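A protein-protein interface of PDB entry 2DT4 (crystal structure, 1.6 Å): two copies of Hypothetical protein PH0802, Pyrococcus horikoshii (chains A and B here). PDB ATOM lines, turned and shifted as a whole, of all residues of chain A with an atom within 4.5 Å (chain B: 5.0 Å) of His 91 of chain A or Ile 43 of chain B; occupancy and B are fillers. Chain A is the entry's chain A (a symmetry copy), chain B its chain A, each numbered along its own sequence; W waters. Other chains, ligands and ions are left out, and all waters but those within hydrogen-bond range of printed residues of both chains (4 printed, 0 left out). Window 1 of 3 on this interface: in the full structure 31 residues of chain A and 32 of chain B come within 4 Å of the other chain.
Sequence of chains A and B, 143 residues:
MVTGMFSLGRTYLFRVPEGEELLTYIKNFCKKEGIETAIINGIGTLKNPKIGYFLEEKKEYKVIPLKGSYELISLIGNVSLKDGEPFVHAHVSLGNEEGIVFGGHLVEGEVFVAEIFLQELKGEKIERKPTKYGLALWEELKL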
ATOM      1  N   SER A  74     -13.176  13.162  12.324  1.00  0.00           N
ATOM      2  CA  SER A  74     -13.528  11.827  12.771  1.00  0.00           C
ATOM      3  C   SER A  74     -13.143  11.655  14.202  1.00  0.00           C
ATOM      4  O   SER A  74     -12.088  12.080  14.571  1.00  0.00           O
ATOM      5  CB  SER A  74     -12.841  10.745  11.935  1.00  0.00           C
ATOM      6  OG  SER A  74     -11.436  10.747  12.067  1.00  0.00           O
ATOM      7  N   LEU A  75     -14.111  10.911  14.917  1.00  0.00           N
ATOM      8  CA  LEU A  75     -13.778  10.434  16.202  1.00  0.00           C
ATOM      9  C   LEU A  75     -14.202   9.002  16.059  1.00  0.00           C
ATOM     10  O   LEU A  75     -15.316   8.733  15.640  1.00  0.00           O
ATOM     11  CB  LEU A  75     -14.566  11.124  17.331  1.00  0.00           C
ATOM     12  CG  LEU A  75     -14.199  10.426  18.646  1.00  0.00           C
ATOM     13  CD1 LEU A  75     -14.018  11.404  19.747  1.00  0.00           C
ATOM     14  CD2 LEU A  75     -15.125   9.311  18.971  1.00  0.00           C
ATOM     15  N   ILE A  76     -13.305   8.084  16.429  1.00  0.00           N
ATOM     16  CA  ILE A  76     -13.615   6.666  16.365  1.00  0.00           C
ATOM     17  C   ILE A  76     -13.010   6.133  17.617  1.00  0.00           C
ATOM     18  O   ILE A  76     -11.885   6.472  17.945  1.00  0.00           O
ATOM     19  CB  ILE A  76     -13.063   5.897  15.148  1.00  0.00           C
ATOM     20  CG1 ILE A  76     -13.672   6.455  13.850  1.00  0.00           C
ATOM     21  CG2 ILE A  76     -13.366   4.433  15.281  1.00  0.00           C
ATOM     22  CD1 ILE A  76     -13.089   5.857  12.630  1.00  0.00           C
ATOM     23  N   GLY A  77     -13.731   5.296  18.330  1.00  0.00           N
ATOM     24  CA  GLY A  77     -13.146   4.713  19.510  1.00  0.00           C
ATOM     25  C   GLY A  77     -14.052   3.746  20.219  1.00  0.00           C
ATOM     26  O   GLY A  77     -15.001   3.233  19.650  1.00  0.00           O
ATOM     27  N   ASN A  78     -13.741   3.511  21.486  1.00  0.00           N
ATOM     28  CA  ASN A  78     -14.486   2.518  22.233  1.00  0.00           C
ATOM     29  C   ASN A  78     -14.490   2.847  23.719  1.00  0.00           C
ATOM     30  O   ASN A  78     -13.705   3.665  24.199  1.00  0.00           O
ATOM     31  CB  ASN A  78     -13.900   1.115  21.952  1.00  0.00           C
ATOM     32  CG  ASN A  78     -12.425   1.035  22.227  1.00  0.00           C
ATOM     33  OD1 ASN A  78     -12.005   1.245  23.372  1.00  0.00           O
ATOM     34  ND2 ASN A  78     -11.615   0.791  21.175  1.00  0.00           N
ATOM     35  N   HIS A  89     -11.423   5.321  24.996  1.00  0.00           N
ATOM     36  CA  HIS A  89     -10.217   5.377  24.169  1.00  0.00           C
ATOM     37  C   HIS A  89     -10.653   5.762  22.783  1.00  0.00           C
ATOM     38  O   HIS A  89     -11.444   5.057  22.169  1.00  0.00           O
ATOM     39  CB  HIS A  89      -9.473   4.054  24.161  1.00  0.00           C
ATOM     40  CG  HIS A  89      -8.154   4.108  23.467  1.00  0.00           C
ATOM     41  ND1 HIS A  89      -7.308   5.195  23.578  1.00  0.00           N
ATOM     42  CD2 HIS A  89      -7.545   3.238  22.622  1.00  0.00           C
ATOM     43  CE1 HIS A  89      -6.221   4.975  22.852  1.00  0.00           C
ATOM     44  NE2 HIS A  89      -6.337   3.793  22.275  1.00  0.00           N
ATOM     45  N   ALA A  90     -10.158   6.891  22.295  1.00  0.00           N
ATOM     46  CA  ALA A  90     -10.514   7.344  20.954  1.00  0.00           C
ATOM     47  C   ALA A  90      -9.380   8.030  20.226  1.00  0.00           C
ATOM     48  O   ALA A  90      -8.477   8.581  20.834  1.00  0.00           O
ATOM     49  CB  ALA A  90     -11.701   8.277  21.006  1.00  0.00           C
ATOM     50  N   HIS A  91      -9.454   8.014  18.903  1.00  0.00           N
ATOM     51  CA  HIS A  91      -8.511   8.722  18.027  1.00  0.00           C
ATOM     52  C   HIS A  91      -9.308   9.720  17.221  1.00  0.00           C
ATOM     53  O   HIS A  91     -10.487   9.512  16.949  1.00  0.00           O
ATOM     54  CB  HIS A  91      -7.787   7.782  17.059  1.00  0.00           C
ATOM     55  CG  HIS A  91      -6.719   6.958  17.711  1.00  0.00           C
ATOM     56  ND1 HIS A  91      -5.444   6.871  17.205  1.00  0.00           N
ATOM     57  CD2 HIS A  91      -6.716   6.239  18.856  1.00  0.00           C
ATOM     58  CE1 HIS A  91      -4.720   6.072  17.970  1.00  0.00           C
ATOM     59  NE2 HIS A  91      -5.467   5.672  18.979  1.00  0.00           N
ATOM     60  N   VAL A  92      -8.646  10.834  16.907  1.00  0.00           N
ATOM     61  CA  VAL A  92      -9.353  11.913  16.172  1.00  0.00           C
ATOM     62  C   VAL A  92      -8.530  12.413  15.007  1.00  0.00           C
ATOM     63  O   VAL A  92      -7.302  12.408  15.040  1.00  0.00           O
ATOM     64  CB  VAL A  92      -9.667  13.110  17.109  1.00  0.00           C
ATOM     65  CG1 VAL A  92     -10.740  12.758  18.105  1.00  0.00           C
ATOM     66  CG2 VAL A  92      -8.402  13.630  17.771  1.00  0.00           C
ATOM     67  N   GLY A 104      -4.353  11.989  15.920  1.00  0.00           N
ATOM     68  CA  GLY A 104      -3.685  10.984  16.706  1.00  0.00           C
ATOM     69  C   GLY A 104      -4.647  10.475  17.761  1.00  0.00           C
ATOM     70  O   GLY A 104      -5.865  10.635  17.628  1.00  0.00           O
ATOM     71  N   HIS A 105      -4.116   9.917  18.844  1.00  0.00           N
ATOM     72  CA  HIS A 105      -4.919   9.551  19.997  1.00  0.00           C
ATOM     73  C   HIS A 105      -5.484  10.820  20.624  1.00  0.00           C
ATOM     74  O   HIS A 105      -4.762  11.803  20.766  1.00  0.00           O
ATOM     75  CB  HIS A 105      -4.013   8.817  20.985  1.00  0.00           C
ATOM     76  CG  HIS A 105      -4.562   8.722  22.369  1.00  0.00           C
ATOM     77  ND1 HIS A 105      -3.867   9.144  23.481  1.00  0.00           N
ATOM     78  CD2 HIS A 105      -5.736   8.225  22.821  1.00  0.00           C
ATOM     79  CE1 HIS A 105      -4.595   8.904  24.556  1.00  0.00           C
ATOM     80  NE2 HIS A 105      -5.730   8.342  24.182  1.00  0.00           N
ATOM     81  N   LEU A 106      -6.753  10.826  21.045  1.00  0.00           N
ATOM     82  CA  LEU A 106      -7.313  11.994  21.700  1.00  0.00           C
ATOM     83  C   LEU A 106      -6.952  11.957  23.179  1.00  0.00           C
ATOM     84  O   LEU A 106      -7.340  11.051  23.890  1.00  0.00           O
ATOM     85  CB  LEU A 106      -8.833  12.055  21.560  1.00  0.00           C
ATOM     86  CG  LEU A 106      -9.471  13.290  22.187  1.00  0.00           C
ATOM     87  CD1 LEU A 106      -9.001  14.592  21.543  1.00  0.00           C
ATOM     88  CD2 LEU A 106     -10.983  13.157  22.125  1.00  0.00           C
ATOM     89  N   ASN B  41     -14.732  -0.808  11.530  1.00  0.00           N
ATOM     90  CA  ASN B  41     -14.208   0.497  11.932  1.00  0.00           C
ATOM     91  C   ASN B  41     -13.154   0.145  12.961  1.00  0.00           C
ATOM     92  O   ASN B  41     -13.245  -0.891  13.599  1.00  0.00           O
ATOM     93  CB  ASN B  41     -15.189   1.576  12.373  1.00  0.00           C
ATOM     94  CG  ASN B  41     -15.551   1.520  13.829  1.00  0.00           C
ATOM     95  OD1 ASN B  41     -14.717   1.268  14.704  1.00  0.00           O
ATOM     96  ND2 ASN B  41     -16.809   1.792  14.101  1.00  0.00           N
ATOM     97  N   GLY B  42     -12.123   0.954  13.081  1.00  0.00           N
ATOM     98  CA  GLY B  42     -11.173   0.741  14.143  1.00  0.00           C
ATOM     99  C   GLY B  42     -10.085   1.790  14.250  1.00  0.00           C
ATOM    100  O   GLY B  42     -10.027   2.732  13.471  1.00  0.00           O
ATOM    101  N   ILE B  43      -9.274   1.590  15.282  1.00  0.00           N
ATOM    102  CA  ILE B  43      -8.163   2.453  15.657  1.00  0.00           C
ATOM    103  C   ILE B  43      -7.001   1.603  16.142  1.00  0.00           C
ATOM    104  O   ILE B  43      -7.125   0.399  16.386  1.00  0.00           O
ATOM    105  CB  ILE B  43      -8.586   3.458  16.777  1.00  0.00           C
ATOM    106  CG1 ILE B  43      -9.059   2.741  18.048  1.00  0.00           C
ATOM    107  CG2 ILE B  43      -9.673   4.450  16.253  1.00  0.00           C
ATOM    108  CD1 ILE B  43      -9.359   3.678  19.224  1.00  0.00           C
ATOM    109  N   GLY B  44      -5.877   2.256  16.333  1.00  0.00           N
ATOM    110  CA  GLY B  44      -4.715   1.631  16.927  1.00  0.00           C
ATOM    111  C   GLY B  44      -3.450   2.272  16.429  1.00  0.00           C
ATOM    112  O   GLY B  44      -3.362   3.501  16.420  1.00  0.00           O
ATOM    113  N   THR B  45      -2.467   1.435  16.096  1.00  0.00           N
ATOM    114  CA  THR B  45      -1.179   1.842  15.514  1.00  0.00           C
ATOM    115  C   THR B  45      -0.719   0.772  14.533  1.00  0.00           C
ATOM    116  O   THR B  45      -0.741  -0.429  14.841  1.00  0.00           O
ATOM    117  CB  THR B  45      -0.140   2.009  16.610  1.00  0.00           C
ATOM    118  OG1 THR B  45      -0.335   3.282  17.246  1.00  0.00           O
ATOM    119  CG2 THR B  45       1.248   2.141  16.036  1.00  0.00           C
ATOM    120  N   GLU B  71       0.025   6.324  14.134  1.00  0.00           N
ATOM    121  CA  GLU B  71      -1.253   6.179  14.827  1.00  0.00           C
ATOM    122  C   GLU B  71      -2.357   5.906  13.781  1.00  0.00           C
ATOM    123  O   GLU B  71      -2.492   6.631  12.770  1.00  0.00           O
ATOM    124  CB  GLU B  71      -1.611   7.399  15.698  1.00  0.00           C
ATOM    125  CG  GLU B  71      -0.643   7.632  16.856  1.00  0.00           C
ATOM    126  CD  GLU B  71      -0.787   6.648  18.006  1.00  0.00           C
ATOM    127  OE1 GLU B  71       0.200   6.414  18.745  1.00  0.00           O
ATOM    128  OE2 GLU B  71      -1.888   6.102  18.238  1.00  0.00           O
ATOM    129  N   LEU B  72      -3.115   4.845  14.003  1.00  0.00           N
ATOM    130  CA  LEU B  72      -4.231   4.485  13.138  1.00  0.00           C
ATOM    131  C   LEU B  72      -5.431   5.277  13.644  1.00  0.00           C
ATOM    132  O   LEU B  72      -6.105   4.876  14.570  1.00  0.00           O
ATOM    133  CB  LEU B  72      -4.457   2.965  13.216  1.00  0.00           C
ATOM    134  CG  LEU B  72      -5.120   2.158  12.071  1.00  0.00           C
ATOM    135  CD1 LEU B  72      -5.926   0.976  12.534  1.00  0.00           C
ATOM    136  CD2 LEU B  72      -5.658   2.885  10.854  1.00  0.00           C
ATOM    137  N   ILE B  73      -5.628   6.456  13.054  1.00  0.00           N
ATOM    138  CA  ILE B  73      -6.621   7.406  13.509  1.00  0.00           C
ATOM    139  C   ILE B  73      -8.015   6.957  13.102  1.00  0.00           C
ATOM    140  O   ILE B  73      -8.942   6.990  13.904  1.00  0.00           O
ATOM    141  CB  ILE B  73      -6.308   8.802  12.954  1.00  0.00           C
ATOM    142  CG1 ILE B  73      -4.999   9.326  13.547  1.00  0.00           C
ATOM    143  CG2 ILE B  73      -7.519   9.775  13.082  1.00  0.00           C
ATOM    144  CD1 ILE B  73      -4.437  10.531  12.831  1.00  0.00           C
ATOM    145  N   VAL B 113      -1.048  -2.324  17.505  1.00  0.00           N
ATOM    146  CA  VAL B 113      -2.312  -2.461  18.269  1.00  0.00           C
ATOM    147  C   VAL B 113      -3.381  -2.151  17.235  1.00  0.00           C
ATOM    148  O   VAL B 113      -3.269  -1.179  16.531  1.00  0.00           O
ATOM    149  CB  VAL B 113      -2.460  -1.493  19.445  1.00  0.00           C
ATOM    150  CG1 VAL B 113      -3.907  -1.509  20.062  1.00  0.00           C
ATOM    151  CG2 VAL B 113      -1.403  -1.820  20.511  1.00  0.00           C
ATOM    152  N   ALA B 114      -4.477  -2.935  17.245  1.00  0.00           N
ATOM    153  CA  ALA B 114      -5.611  -2.622  16.343  1.00  0.00           C
ATOM    154  C   ALA B 114      -6.854  -3.106  17.093  1.00  0.00           C
ATOM    155  O   ALA B 114      -6.939  -4.300  17.468  1.00  0.00           O
ATOM    156  CB  ALA B 114      -5.561  -3.203  14.957  1.00  0.00           C
ATOM    157  N   GLU B 115      -7.768  -2.175  17.339  1.00  0.00           N
ATOM    158  CA  GLU B 115      -8.985  -2.407  18.067  1.00  0.00           C
ATOM    159  C   GLU B 115     -10.064  -2.208  17.023  1.00  0.00           C
ATOM    160  O   GLU B 115     -10.343  -1.075  16.582  1.00  0.00           O
ATOM    161  CB  GLU B 115      -9.117  -1.458  19.259  1.00  0.00           C
ATOM    162  CG  GLU B 115      -8.039  -1.746  20.302  1.00  0.00           C
ATOM    163  CD  GLU B 115      -7.923  -0.725  21.415  1.00  0.00           C
ATOM    164  OE1 GLU B 115      -8.653   0.281  21.440  1.00  0.00           O
ATOM    165  OE2 GLU B 115      -7.046  -0.910  22.290  1.00  0.00           O
ATOM    166  N   ILE B 116     -10.566  -3.342  16.567  1.00  0.00           N
ATOM    167  CA  ILE B 116     -11.524  -3.392  15.469  1.00  0.00           C
ATOM    168  C   ILE B 116     -12.957  -3.778  15.890  1.00  0.00           C
ATOM    169  O   ILE B 116     -13.163  -4.751  16.663  1.00  0.00           O
ATOM    170  CB  ILE B 116     -10.991  -4.455  14.460  1.00  0.00           C
ATOM    171  CG1 ILE B 116      -9.552  -4.162  13.969  1.00  0.00           C
ATOM    172  CG2 ILE B 116     -11.953  -4.611  13.301  1.00  0.00           C
ATOM    173  CD1 ILE B 116      -9.276  -2.784  13.415  1.00  0.00           C
HETATM  174  O   HOH W   1      -5.028   0.843  22.509  1.00  0.00           O
HETATM  175  O   HOH W   2     -14.519   1.403  17.262  1.00  0.00           O
HETATM  176  O   HOH W   3     -12.308   0.314  18.412  1.00  0.00           O
HETATM  177  O   HOH W   4     -10.882   8.989  14.066  1.00  0.00           O
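O of Leu 72 of chain B is in hydrogen-bond range of ND1 of His 91 of chain A (3.4 Å). The side-chain carboxylate of Glu 115 of chain B lies within hydrogen-bond range of the side-chain amide nitrogen of Asn 78 of chain A.
N of His 91 of chain A lies within hydrogen-bond range of O of Ile 76 of chain A, at 3.0 Å. The backbone NH (N) of Val 92 of chain A is in hydrogen-bond range of the backbone carbonyl oxygen (O) of Gly 104 of chain A (2.9 Å). N of Asn 78 of chain A lies within hydrogen-bond range of O of His 89 of chain A (2.9 Å). The backbone carbonyl oxygen of Ile 43 of chain B is in hydrogen-bond range of the backbone NH of Glu 115 of chain B, 2.8 Å away. N of Leu 72 of chain B is in hydrogen-bond range of O of Gly 44 of chain B. The side-chain carboxylate of Glu 71 of chain B sits at hydrogen-bond distance from the side-chain hydroxyl of Thr 45 of chain B (3.4 Å).
Among the printed residues, merely in contact across the chains: His 91 of chain A with Glu 71 of chain B (2.8 Å), Val 92 of chain A with Ile 73 of chain B (3.3 Å), His 91 of chain A with Gly 44 of chain B (3.3 Å), His 89 of chain A with Glu 115 of chain B (3.4 Å), Gly 104 of chain A with Ile 73 of chain B (3.4 Å), Ile 76 of chain A with Ile 43 of chain B (3.4 Å), His 91 of chain A with Ile 73 of chain B (3.5 Å), Ile 76 of chain A with Asn 41 of chain B (3.5 Å), His 91 of chain A with Ile 43 of chain B (3.7 Å), His 89 of chain A with Ile 43 of chain B (3.9 Å) and Gly 77 of chain A with Ile 43 of chain B (3.9 Å).
His 91 of chain A touches just these residues of chain B: Ile 43 (3.7 Å), Gly 44 (3.3 Å), Glu 71 (2.8 Å), Leu 72 (3.4 Å) and Ile 73 (3.5 Å). Of the printed residues of chain A, Glu 71 of chain B touches His 91. Of the printed residues of chain B, His 89 of chain A touches Ile 43 and Glu 115. The nearest printed residue of chain B that does not touch His 91 of chain A is Thr 45 of chain B (5.2 Å). The nearest residue of chain A that does not touch Ile 43 of chain B is Asn 78 of chain A (4.2 Å). The nearest printed residue of chain B that does not touch His 89 of chain A is Gly 44 of chain B (6.0 Å).
Along chain B the printed residues that touch a printed residue of chain A span positions 41 to 115. Among the printed residues, 13 pairs touch across the chains. Among the printed residues, no Asp or Glu carboxylate lies within 4 Å of a Lys or Arg side-chain nitrogen of the other chain.
No position is printed for both chains.
Water W2 lies within hydrogen-bond range of the side-chain amide oxygen of Asn 41 of chain B (2.6 Å) and the backbone carbonyl oxygen of Gly 77 of chain A (3.0 Å). Water W1 lies within hydrogen-bond range of OE2 of Glu 115 of chain B (2.7 Å) and NE2 of His 89 of chain A (3.2 Å). Water W4 lies within hydrogen-bond range of OG of Ser 74 of chain A (2.7 Å), O of Ile 73 of chain B (2.8 Å) and O of His 91 of chain A (3.0 Å). Water W3 bridges ND2 of Asn 78 of chain A and O of Glu 115 of chain B.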
